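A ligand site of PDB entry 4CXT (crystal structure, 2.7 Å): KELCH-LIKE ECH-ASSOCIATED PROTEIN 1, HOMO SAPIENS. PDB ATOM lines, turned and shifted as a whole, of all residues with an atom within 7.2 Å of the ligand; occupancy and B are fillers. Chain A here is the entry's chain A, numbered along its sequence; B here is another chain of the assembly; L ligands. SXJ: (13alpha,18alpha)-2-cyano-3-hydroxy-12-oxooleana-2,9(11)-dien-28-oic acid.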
ATOM      1  N   TYR A  42      11.979  -6.768 -31.527  1.00  0.00           N
ATOM      2  CA  TYR A  42      11.311  -5.655 -30.850  1.00  0.00           C
ATOM      3  C   TYR A  42      11.778  -4.326 -31.430  1.00  0.00           C
ATOM      4  O   TYR A  42      12.988  -4.089 -31.482  1.00  0.00           O
ATOM      5  CB  TYR A  42      11.618  -5.698 -29.342  1.00  0.00           C
ATOM      6  CG  TYR A  42      10.775  -4.757 -28.510  1.00  0.00           C
ATOM      7  CD1 TYR A  42       9.490  -5.109 -28.114  1.00  0.00           C
ATOM      8  CD2 TYR A  42      11.281  -3.530 -28.099  1.00  0.00           C
ATOM      9  CE1 TYR A  42       8.720  -4.242 -27.329  1.00  0.00           C
ATOM     10  CE2 TYR A  42      10.513  -2.661 -27.324  1.00  0.00           C
ATOM     11  CZ  TYR A  42       9.232  -3.027 -26.931  1.00  0.00           C
ATOM     12  OH  TYR A  42       8.470  -2.184 -26.162  1.00  0.00           O
ATOM     13  N   GLN A  43      10.825  -3.465 -31.873  1.00  0.00           N
ATOM     14  CA  GLN A  43      11.037  -2.083 -32.325  1.00  0.00           C
ATOM     15  C   GLN A  43      12.340  -1.893 -33.127  1.00  0.00           C
ATOM     16  O   GLN A  43      12.548  -2.611 -34.112  1.00  0.00           O
ATOM     17  CB  GLN A  43      10.946  -1.113 -31.133  1.00  0.00           C
ATOM     18  CG  GLN A  43       9.511  -0.896 -30.646  1.00  0.00           C
ATOM     19  CD  GLN A  43       9.388   0.112 -29.525  1.00  0.00           C
ATOM     20  OE1 GLN A  43       8.723  -0.125 -28.518  1.00  0.00           O
ATOM     21  NE2 GLN A  43      10.009   1.279 -29.692  1.00  0.00           N
ATOM     22  N   ASP A  44      13.228  -0.978 -32.689  1.00  0.00           N
ATOM     23  CA  ASP A  44      14.523  -0.698 -33.339  1.00  0.00           C
ATOM     24  C   ASP A  44      15.649  -1.642 -32.893  1.00  0.00           C
ATOM     25  O   ASP A  44      16.724  -1.651 -33.516  1.00  0.00           O
ATOM     26  CB  ASP A  44      14.904   0.782 -33.159  1.00  0.00           C
ATOM     27  CG  ASP A  44      14.021   1.752 -33.926  1.00  0.00           C
ATOM     28  OD1 ASP A  44      12.780   1.577 -33.884  1.00  0.00           O
ATOM     29  OD2 ASP A  44      14.576   2.676 -34.564  1.00  0.00           O
ATOM     30  N   ALA A  45      15.414  -2.448 -31.828  1.00  0.00           N
ATOM     31  CA  ALA A  45      16.376  -3.400 -31.272  1.00  0.00           C
ATOM     32  C   ALA A  45      16.819  -4.440 -32.288  1.00  0.00           C
ATOM     33  O   ALA A  45      15.978  -4.910 -33.064  1.00  0.00           O
ATOM     34  CB  ALA A  45      15.799  -4.100 -30.051  1.00  0.00           C
ATOM     35  N   ILE A  85       8.053  -8.158 -26.839  1.00  0.00           N
ATOM     36  CA  ILE A  85       9.047  -8.228 -25.761  1.00  0.00           C
ATOM     37  C   ILE A  85      10.407  -7.936 -26.328  1.00  0.00           C
ATOM     38  O   ILE A  85      10.749  -8.432 -27.409  1.00  0.00           O
ATOM     39  CB  ILE A  85       9.081  -9.561 -24.993  1.00  0.00           C
ATOM     40  CG1 ILE A  85       8.142 -10.602 -25.586  1.00  0.00           C
ATOM     41  CG2 ILE A  85       8.818  -9.363 -23.512  1.00  0.00           C
ATOM     42  CD1 ILE A  85       8.646 -11.886 -25.433  1.00  0.00           C
ATOM     43  N   HIS A  86      11.189  -7.114 -25.611  1.00  0.00           N
ATOM     44  CA  HIS A  86      12.580  -6.833 -25.940  1.00  0.00           C
ATOM     45  C   HIS A  86      13.395  -8.131 -25.764  1.00  0.00           C
ATOM     46  O   HIS A  86      13.092  -8.885 -24.838  1.00  0.00           O
ATOM     47  CB  HIS A  86      13.128  -5.700 -25.056  1.00  0.00           C
ATOM     48  CG  HIS A  86      14.477  -5.211 -25.483  1.00  0.00           C
ATOM     49  ND1 HIS A  86      14.622  -4.203 -26.423  1.00  0.00           N
ATOM     50  CD2 HIS A  86      15.705  -5.626 -25.103  1.00  0.00           C
ATOM     51  CE1 HIS A  86      15.924  -4.033 -26.569  1.00  0.00           C
ATOM     52  NE2 HIS A  86      16.618  -4.871 -25.806  1.00  0.00           N
ATOM     53  N   PRO A  87      14.373  -8.420 -26.673  1.00  0.00           N
ATOM     54  CA  PRO A  87      15.233  -9.609 -26.498  1.00  0.00           C
ATOM     55  C   PRO A  87      15.825  -9.844 -25.100  1.00  0.00           C
ATOM     56  O   PRO A  87      15.929 -10.995 -24.679  1.00  0.00           O
ATOM     57  CB  PRO A  87      16.332  -9.381 -27.527  1.00  0.00           C
ATOM     58  CG  PRO A  87      15.657  -8.662 -28.619  1.00  0.00           C
ATOM     59  CD  PRO A  87      14.690  -7.738 -27.947  1.00  0.00           C
ATOM     60  N   LYS A  88      16.216  -8.761 -24.395  1.00  0.00           N
ATOM     61  CA  LYS A  88      16.758  -8.835 -23.036  1.00  0.00           C
ATOM     62  C   LYS A  88      15.722  -9.357 -22.026  1.00  0.00           C
ATOM     63  O   LYS A  88      16.089 -10.124 -21.134  1.00  0.00           O
ATOM     64  CB  LYS A  88      17.360  -7.495 -22.591  1.00  0.00           C
ATOM     65  N   VAL A  89      14.446  -8.987 -22.206  1.00  0.00           N
ATOM     66  CA  VAL A  89      13.334  -9.507 -21.383  1.00  0.00           C
ATOM     67  C   VAL A  89      13.109 -10.993 -21.657  1.00  0.00           C
ATOM     68  O   VAL A  89      13.099 -11.788 -20.709  1.00  0.00           O
ATOM     69  CB  VAL A  89      12.022  -8.668 -21.465  1.00  0.00           C
ATOM     70  CG1 VAL A  89      10.954  -9.263 -20.558  1.00  0.00           C
ATOM     71  CG2 VAL A  89      12.270  -7.216 -21.088  1.00  0.00           C
ATOM     72  N   GLU A  91      15.234 -13.127 -22.850  1.00  0.00           N
ATOM     73  CA  GLU A  91      16.409 -13.799 -22.292  1.00  0.00           C
ATOM     74  C   GLU A  91      16.231 -14.121 -20.805  1.00  0.00           C
ATOM     75  O   GLU A  91      16.470 -15.266 -20.416  1.00  0.00           O
ATOM     76  CB  GLU A  91      17.654 -12.960 -22.510  1.00  0.00           C
ATOM     77  CG  GLU A  91      18.940 -13.658 -22.137  1.00  0.00           C
ATOM     78  CD  GLU A  91      20.128 -12.754 -22.307  1.00  0.00           C
ATOM     79  OE1 GLU A  91      20.324 -11.857 -21.445  1.00  0.00           O
ATOM     80  OE2 GLU A  91      20.825 -12.878 -23.338  1.00  0.00           O
ATOM     81  N   ARG A  92      15.789 -13.146 -19.989  1.00  0.00           N
ATOM     82  CA  ARG A  92      15.600 -13.338 -18.553  1.00  0.00           C
ATOM     83  C   ARG A  92      14.523 -14.353 -18.199  1.00  0.00           C
ATOM     84  O   ARG A  92      14.701 -15.096 -17.236  1.00  0.00           O
ATOM     85  CB  ARG A  92      15.346 -12.002 -17.855  1.00  0.00           C
ATOM     86  CG  ARG A  92      16.631 -11.392 -17.343  1.00  0.00           C
ATOM     87  CD  ARG A  92      16.870 -10.008 -17.895  1.00  0.00           C
ATOM     88  NE  ARG A  92      18.161  -9.485 -17.450  1.00  0.00           N
ATOM     89  CZ  ARG A  92      19.166  -9.168 -18.261  1.00  0.00           C
ATOM     90  NH1 ARG A  92      19.047  -9.302 -19.575  1.00  0.00           N
ATOM     91  NH2 ARG A  92      20.298  -8.686 -17.757  1.00  0.00           N
ATOM     92  N   SER A 103      16.941 -12.049 -12.806  1.00  0.00           N
ATOM     93  CA  SER A 103      17.645 -10.862 -12.330  1.00  0.00           C
ATOM     94  C   SER A 103      17.443  -9.673 -13.274  1.00  0.00           C
ATOM     95  O   SER A 103      17.520  -9.830 -14.497  1.00  0.00           O
ATOM     96  CB  SER A 103      19.128 -11.150 -12.143  1.00  0.00           C
ATOM     97  OG  SER A 103      19.852  -9.977 -11.806  1.00  0.00           O
ATOM     98  N   MET A 104      17.203  -8.491 -12.703  1.00  0.00           N
ATOM     99  CA  MET A 104      16.994  -7.246 -13.451  1.00  0.00           C
ATOM    100  C   MET A 104      17.351  -6.039 -12.578  1.00  0.00           C
ATOM    101  O   MET A 104      17.283  -6.128 -11.351  1.00  0.00           O
ATOM    102  CB  MET A 104      15.534  -7.147 -13.986  1.00  0.00           C
ATOM    103  CG  MET A 104      14.472  -6.905 -12.907  1.00  0.00           C
ATOM    104  SD  MET A 104      13.103  -8.095 -12.830  1.00  0.00           S
ATOM    105  CE  MET A 104      13.909  -9.485 -12.086  1.00  0.00           C
ATOM    106  N   GLY A 105      17.746  -4.939 -13.221  1.00  0.00           N
ATOM    107  CA  GLY A 105      17.869  -3.647 -12.558  1.00  0.00           C
ATOM    108  C   GLY A 105      16.502  -3.108 -12.217  1.00  0.00           C
ATOM    109  O   GLY A 105      15.535  -3.383 -12.943  1.00  0.00           O
ATOM    110  N   GLU A 106      16.386  -2.332 -11.120  1.00  0.00           N
ATOM    111  CA  GLU A 106      15.105  -1.889 -10.564  1.00  0.00           C
ATOM    112  C   GLU A 106      14.254  -1.048 -11.543  1.00  0.00           C
ATOM    113  O   GLU A 106      13.023  -1.034 -11.401  1.00  0.00           O
ATOM    114  CB  GLU A 106      15.278  -1.165  -9.214  1.00  0.00           C
ATOM    115  CG  GLU A 106      16.138   0.088  -9.227  1.00  0.00           C
ATOM    116  CD  GLU A 106      15.906   1.002  -8.051  1.00  0.00           C
ATOM    117  OE1 GLU A 106      14.899   1.749  -8.069  1.00  0.00           O
ATOM    118  OE2 GLU A 106      16.725   0.985  -7.104  1.00  0.00           O
ATOM    119  N   LYS A 107      14.888  -0.394 -12.541  1.00  0.00           N
ATOM    120  CA  LYS A 107      14.165   0.441 -13.515  1.00  0.00           C
ATOM    121  C   LYS A 107      13.413  -0.390 -14.569  1.00  0.00           C
ATOM    122  O   LYS A 107      12.549   0.149 -15.267  1.00  0.00           O
ATOM    123  CB  LYS A 107      15.084   1.508 -14.167  1.00  0.00           C
ATOM    124  CG  LYS A 107      16.246   0.972 -15.001  1.00  0.00           C
ATOM    125  CD  LYS A 107      16.674   1.949 -16.099  1.00  0.00           C
ATOM    126  CE  LYS A 107      17.890   1.447 -16.858  1.00  0.00           C
ATOM    127  NZ  LYS A 107      18.048   2.119 -18.170  1.00  0.00           N
ATOM    128  N   CYS A 108      13.708  -1.700 -14.663  1.00  0.00           N
ATOM    129  CA  CYS A 108      13.101  -2.562 -15.683  1.00  0.00           C
ATOM    130  C   CYS A 108      12.300  -3.727 -15.118  1.00  0.00           C
ATOM    131  O   CYS A 108      11.957  -4.643 -15.870  1.00  0.00           O
ATOM    132  CB  CYS A 108      14.158  -3.029 -16.669  1.00  0.00           C
ATOM    133  SG  CYS A 108      14.884  -1.630 -17.577  1.00  0.00           S
ATOM    134  N   VAL A 109      11.963  -3.693 -13.819  1.00  0.00           N
ATOM    135  CA  VAL A 109      11.055  -4.629 -13.137  1.00  0.00           C
ATOM    136  C   VAL A 109       9.679  -4.594 -13.821  1.00  0.00           C
ATOM    137  O   VAL A 109       9.052  -5.643 -14.004  1.00  0.00           O
ATOM    138  CB  VAL A 109      11.007  -4.334 -11.611  1.00  0.00           C
ATOM    139  CG1 VAL A 109       9.947  -5.152 -10.896  1.00  0.00           C
ATOM    140  CG2 VAL A 109      12.375  -4.551 -10.960  1.00  0.00           C
ATOM    141  N   HIS A 111       9.027  -3.894 -17.069  1.00  0.00           N
ATOM    142  CA  HIS A 111       9.104  -4.448 -18.419  1.00  0.00           C
ATOM    143  C   HIS A 111       9.226  -5.985 -18.406  1.00  0.00           C
ATOM    144  O   HIS A 111       8.713  -6.656 -19.306  1.00  0.00           O
ATOM    145  CB  HIS A 111      10.248  -3.782 -19.192  1.00  0.00           C
ATOM    146  CG  HIS A 111      10.193  -2.283 -19.126  1.00  0.00           C
ATOM    147  ND1 HIS A 111       9.201  -1.570 -19.780  1.00  0.00           N
ATOM    148  CD2 HIS A 111      10.956  -1.418 -18.422  1.00  0.00           C
ATOM    149  CE1 HIS A 111       9.415  -0.288 -19.483  1.00  0.00           C
ATOM    150  NE2 HIS A 111      10.468  -0.153 -18.672  1.00  0.00           N
ATOM    151  N   VAL A 112       9.930  -6.514 -17.389  1.00  0.00           N
ATOM    152  CA  VAL A 112      10.010  -7.931 -17.073  1.00  0.00           C
ATOM    153  C   VAL A 112       8.633  -8.446 -16.661  1.00  0.00           C
ATOM    154  O   VAL A 112       8.216  -9.517 -17.123  1.00  0.00           O
ATOM    155  CB  VAL A 112      11.119  -8.234 -16.027  1.00  0.00           C
ATOM    156  CG1 VAL A 112      11.082  -9.695 -15.558  1.00  0.00           C
ATOM    157  CG2 VAL A 112      12.499  -7.889 -16.574  1.00  0.00           C
ATOM    158  N   ASN B   6      18.972   1.990  -9.660  1.00  0.00           N
ATOM    159  CA  ASN B   6      19.948   2.188  -8.593  1.00  0.00           C
ATOM    160  C   ASN B   6      20.316   0.875  -7.861  1.00  0.00           C
ATOM    161  O   ASN B   6      21.289   0.845  -7.106  1.00  0.00           O
ATOM    162  CB  ASN B   6      19.468   3.262  -7.606  1.00  0.00           C
ATOM    163  CG  ASN B   6      19.208   4.640  -8.209  1.00  0.00           C
ATOM    164  OD1 ASN B   6      18.618   4.786  -9.291  1.00  0.00           O
ATOM    165  ND2 ASN B   6      19.578   5.690  -7.487  1.00  0.00           N
ATOM    166  N   ARG B   7      19.556  -0.219  -8.098  1.00  0.00           N
ATOM    167  CA  ARG B   7      19.700  -1.514  -7.433  1.00  0.00           C
ATOM    168  C   ARG B   7      19.430  -2.701  -8.387  1.00  0.00           C
ATOM    169  O   ARG B   7      18.823  -2.525  -9.453  1.00  0.00           O
ATOM    170  CB  ARG B   7      18.730  -1.586  -6.223  1.00  0.00           C
ATOM    171  CG  ARG B   7      19.395  -1.541  -4.854  1.00  0.00           C
ATOM    172  CD  ARG B   7      18.385  -1.585  -3.709  1.00  0.00           C
ATOM    173  NE  ARG B   7      17.761  -2.905  -3.534  1.00  0.00           N
ATOM    174  CZ  ARG B   7      17.962  -3.699  -2.485  1.00  0.00           C
ATOM    175  NH1 ARG B   7      18.770  -3.324  -1.499  1.00  0.00           N
ATOM    176  NH2 ARG B   7      17.347  -4.882  -2.406  1.00  0.00           N
ATOM    177  N   THR B   8      19.890  -3.909  -7.998  1.00  0.00           N
ATOM    178  CA  THR B   8      19.678  -5.160  -8.744  1.00  0.00           C
ATOM    179  C   THR B   8      18.654  -6.032  -8.016  1.00  0.00           C
ATOM    180  O   THR B   8      18.987  -6.677  -7.010  1.00  0.00           O
ATOM    181  CB  THR B   8      21.019  -5.900  -8.990  1.00  0.00           C
ATOM    182  OG1 THR B   8      22.100  -4.978  -9.136  1.00  0.00           O
ATOM    183  CG2 THR B   8      20.954  -6.835 -10.186  1.00  0.00           C
HETATM  184  C1  SXJ L   1      11.695   3.471 -23.484  1.00  0.00           C
HETATM  185  C2  SXJ L   1      11.091   2.125 -23.045  1.00  0.00           C
HETATM  186  C3  SXJ L   1       9.978   2.375 -22.029  1.00  0.00           C
HETATM  187  C4  SXJ L   1      10.519   1.380 -24.268  1.00  0.00           C
HETATM  188  C5  SXJ L   1      11.583   0.904 -25.245  1.00  0.00           C
HETATM  189  C6  SXJ L   1      12.681   0.041 -24.600  1.00  0.00           C
HETATM  190  C7  SXJ L   1      12.137  -1.345 -24.213  1.00  0.00           C
HETATM  191  C8  SXJ L   1      13.194  -2.234 -23.564  1.00  0.00           C
HETATM  192  C9  SXJ L   1      13.884  -1.602 -22.337  1.00  0.00           C
HETATM  193  C10 SXJ L   1      12.886  -1.645 -21.157  1.00  0.00           C
HETATM  194  C11 SXJ L   1      14.350  -0.149 -22.680  1.00  0.00           C
HETATM  195  C13 SXJ L   1      13.280   0.757 -23.348  1.00  0.00           C
HETATM  196  C15 SXJ L   1      12.177   1.243 -22.398  1.00  0.00           C
HETATM  197  C16 SXJ L   1      14.966   0.462 -21.444  1.00  0.00           C
HETATM  198  O17 SXJ L   1      14.878   1.658 -21.208  1.00  0.00           O
HETATM  199  C18 SXJ L   1      15.694  -0.426 -20.527  1.00  0.00           C
HETATM  200  C19 SXJ L   1      15.856  -1.761 -20.691  1.00  0.00           C
HETATM  201  C20 SXJ L   1      15.232  -2.423 -21.944  1.00  0.00           C
HETATM  202  C21 SXJ L   1      16.311  -2.342 -23.041  1.00  0.00           C
HETATM  203  C22 SXJ L   1      14.900  -3.915 -21.732  1.00  0.00           C
HETATM  204  C23 SXJ L   1      15.946  -4.665 -20.927  1.00  0.00           C
HETATM  205  C24 SXJ L   1      16.118  -4.053 -19.546  1.00  0.00           C
HETATM  206  C26 SXJ L   1      16.846  -5.009 -18.532  1.00  0.00           C
HETATM  207  C27 SXJ L   1      15.831  -6.027 -17.973  1.00  0.00           C
HETATM  208  C28 SXJ L   1      17.987  -5.809 -19.192  1.00  0.00           C
HETATM  209  C29 SXJ L   1      17.419  -4.229 -17.363  1.00  0.00           C
HETATM  210  O30 SXJ L   1      18.057  -5.018 -16.491  1.00  0.00           O
HETATM  211  C31 SXJ L   1      17.286  -2.867 -17.217  1.00  0.00           C
HETATM  212  C32 SXJ L   1      16.555  -1.988 -18.222  1.00  0.00           C
HETATM  213  C33 SXJ L   1      16.667  -2.587 -19.663  1.00  0.00           C
HETATM  214  C34 SXJ L   1      18.132  -2.476 -20.110  1.00  0.00           C
HETATM  215  C35 SXJ L   1      17.851  -2.212 -16.097  1.00  0.00           C
HETATM  216  N36 SXJ L   1      18.305  -1.688 -15.179  1.00  0.00           N
HETATM  217  C37 SXJ L   1      13.734  -0.144 -25.739  1.00  0.00           C
HETATM  218  O38 SXJ L   1      14.856   0.396 -25.583  1.00  0.00           O
HETATM  219  O39 SXJ L   1      13.375  -0.820 -26.733  1.00  0.00           O
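Merely in contact with the ligand: Tyr 42 (3.5 Å), His 86 (3.6 Å), Lys 88 (3.6 Å), Arg 92 (3.7 Å), Met 104 (3.9 Å), Lys 107 (3.4 Å) and His 111 (3.4 Å). Hydrophobic or aromatic side chains that line the ligand: Tyr 42, His 86 and His 111. Along chain A the residues within 4 Å of the ligand span positions 42 to 111. The nearest printed residue that does not touch the ligand is Val 112 (4.1 Å).
SG of Cys 108 is bonded to C32 of the ligand, at 1.8 Å. O30 of the ligand sits at hydrogen-bond distance from N of Gly 105.
The side-chain amide oxygen (OE1) of Gln 43 sits at hydrogen-bond distance from the side-chain hydroxyl (OH) of Tyr 42 (3.1 Å). The guanidinium group (NH1) of Arg 92 sits close to the backbone carbonyl oxygen (O) of Lys 88, 3.4 Å away. O of Ser 103 lies within hydrogen-bond range of NE of Arg 92, 3.0 Å away. The guanidinium group (NH1) of Arg 92 lies within salt-bridge range of the side-chain carboxylate (OE1) of Glu 91.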
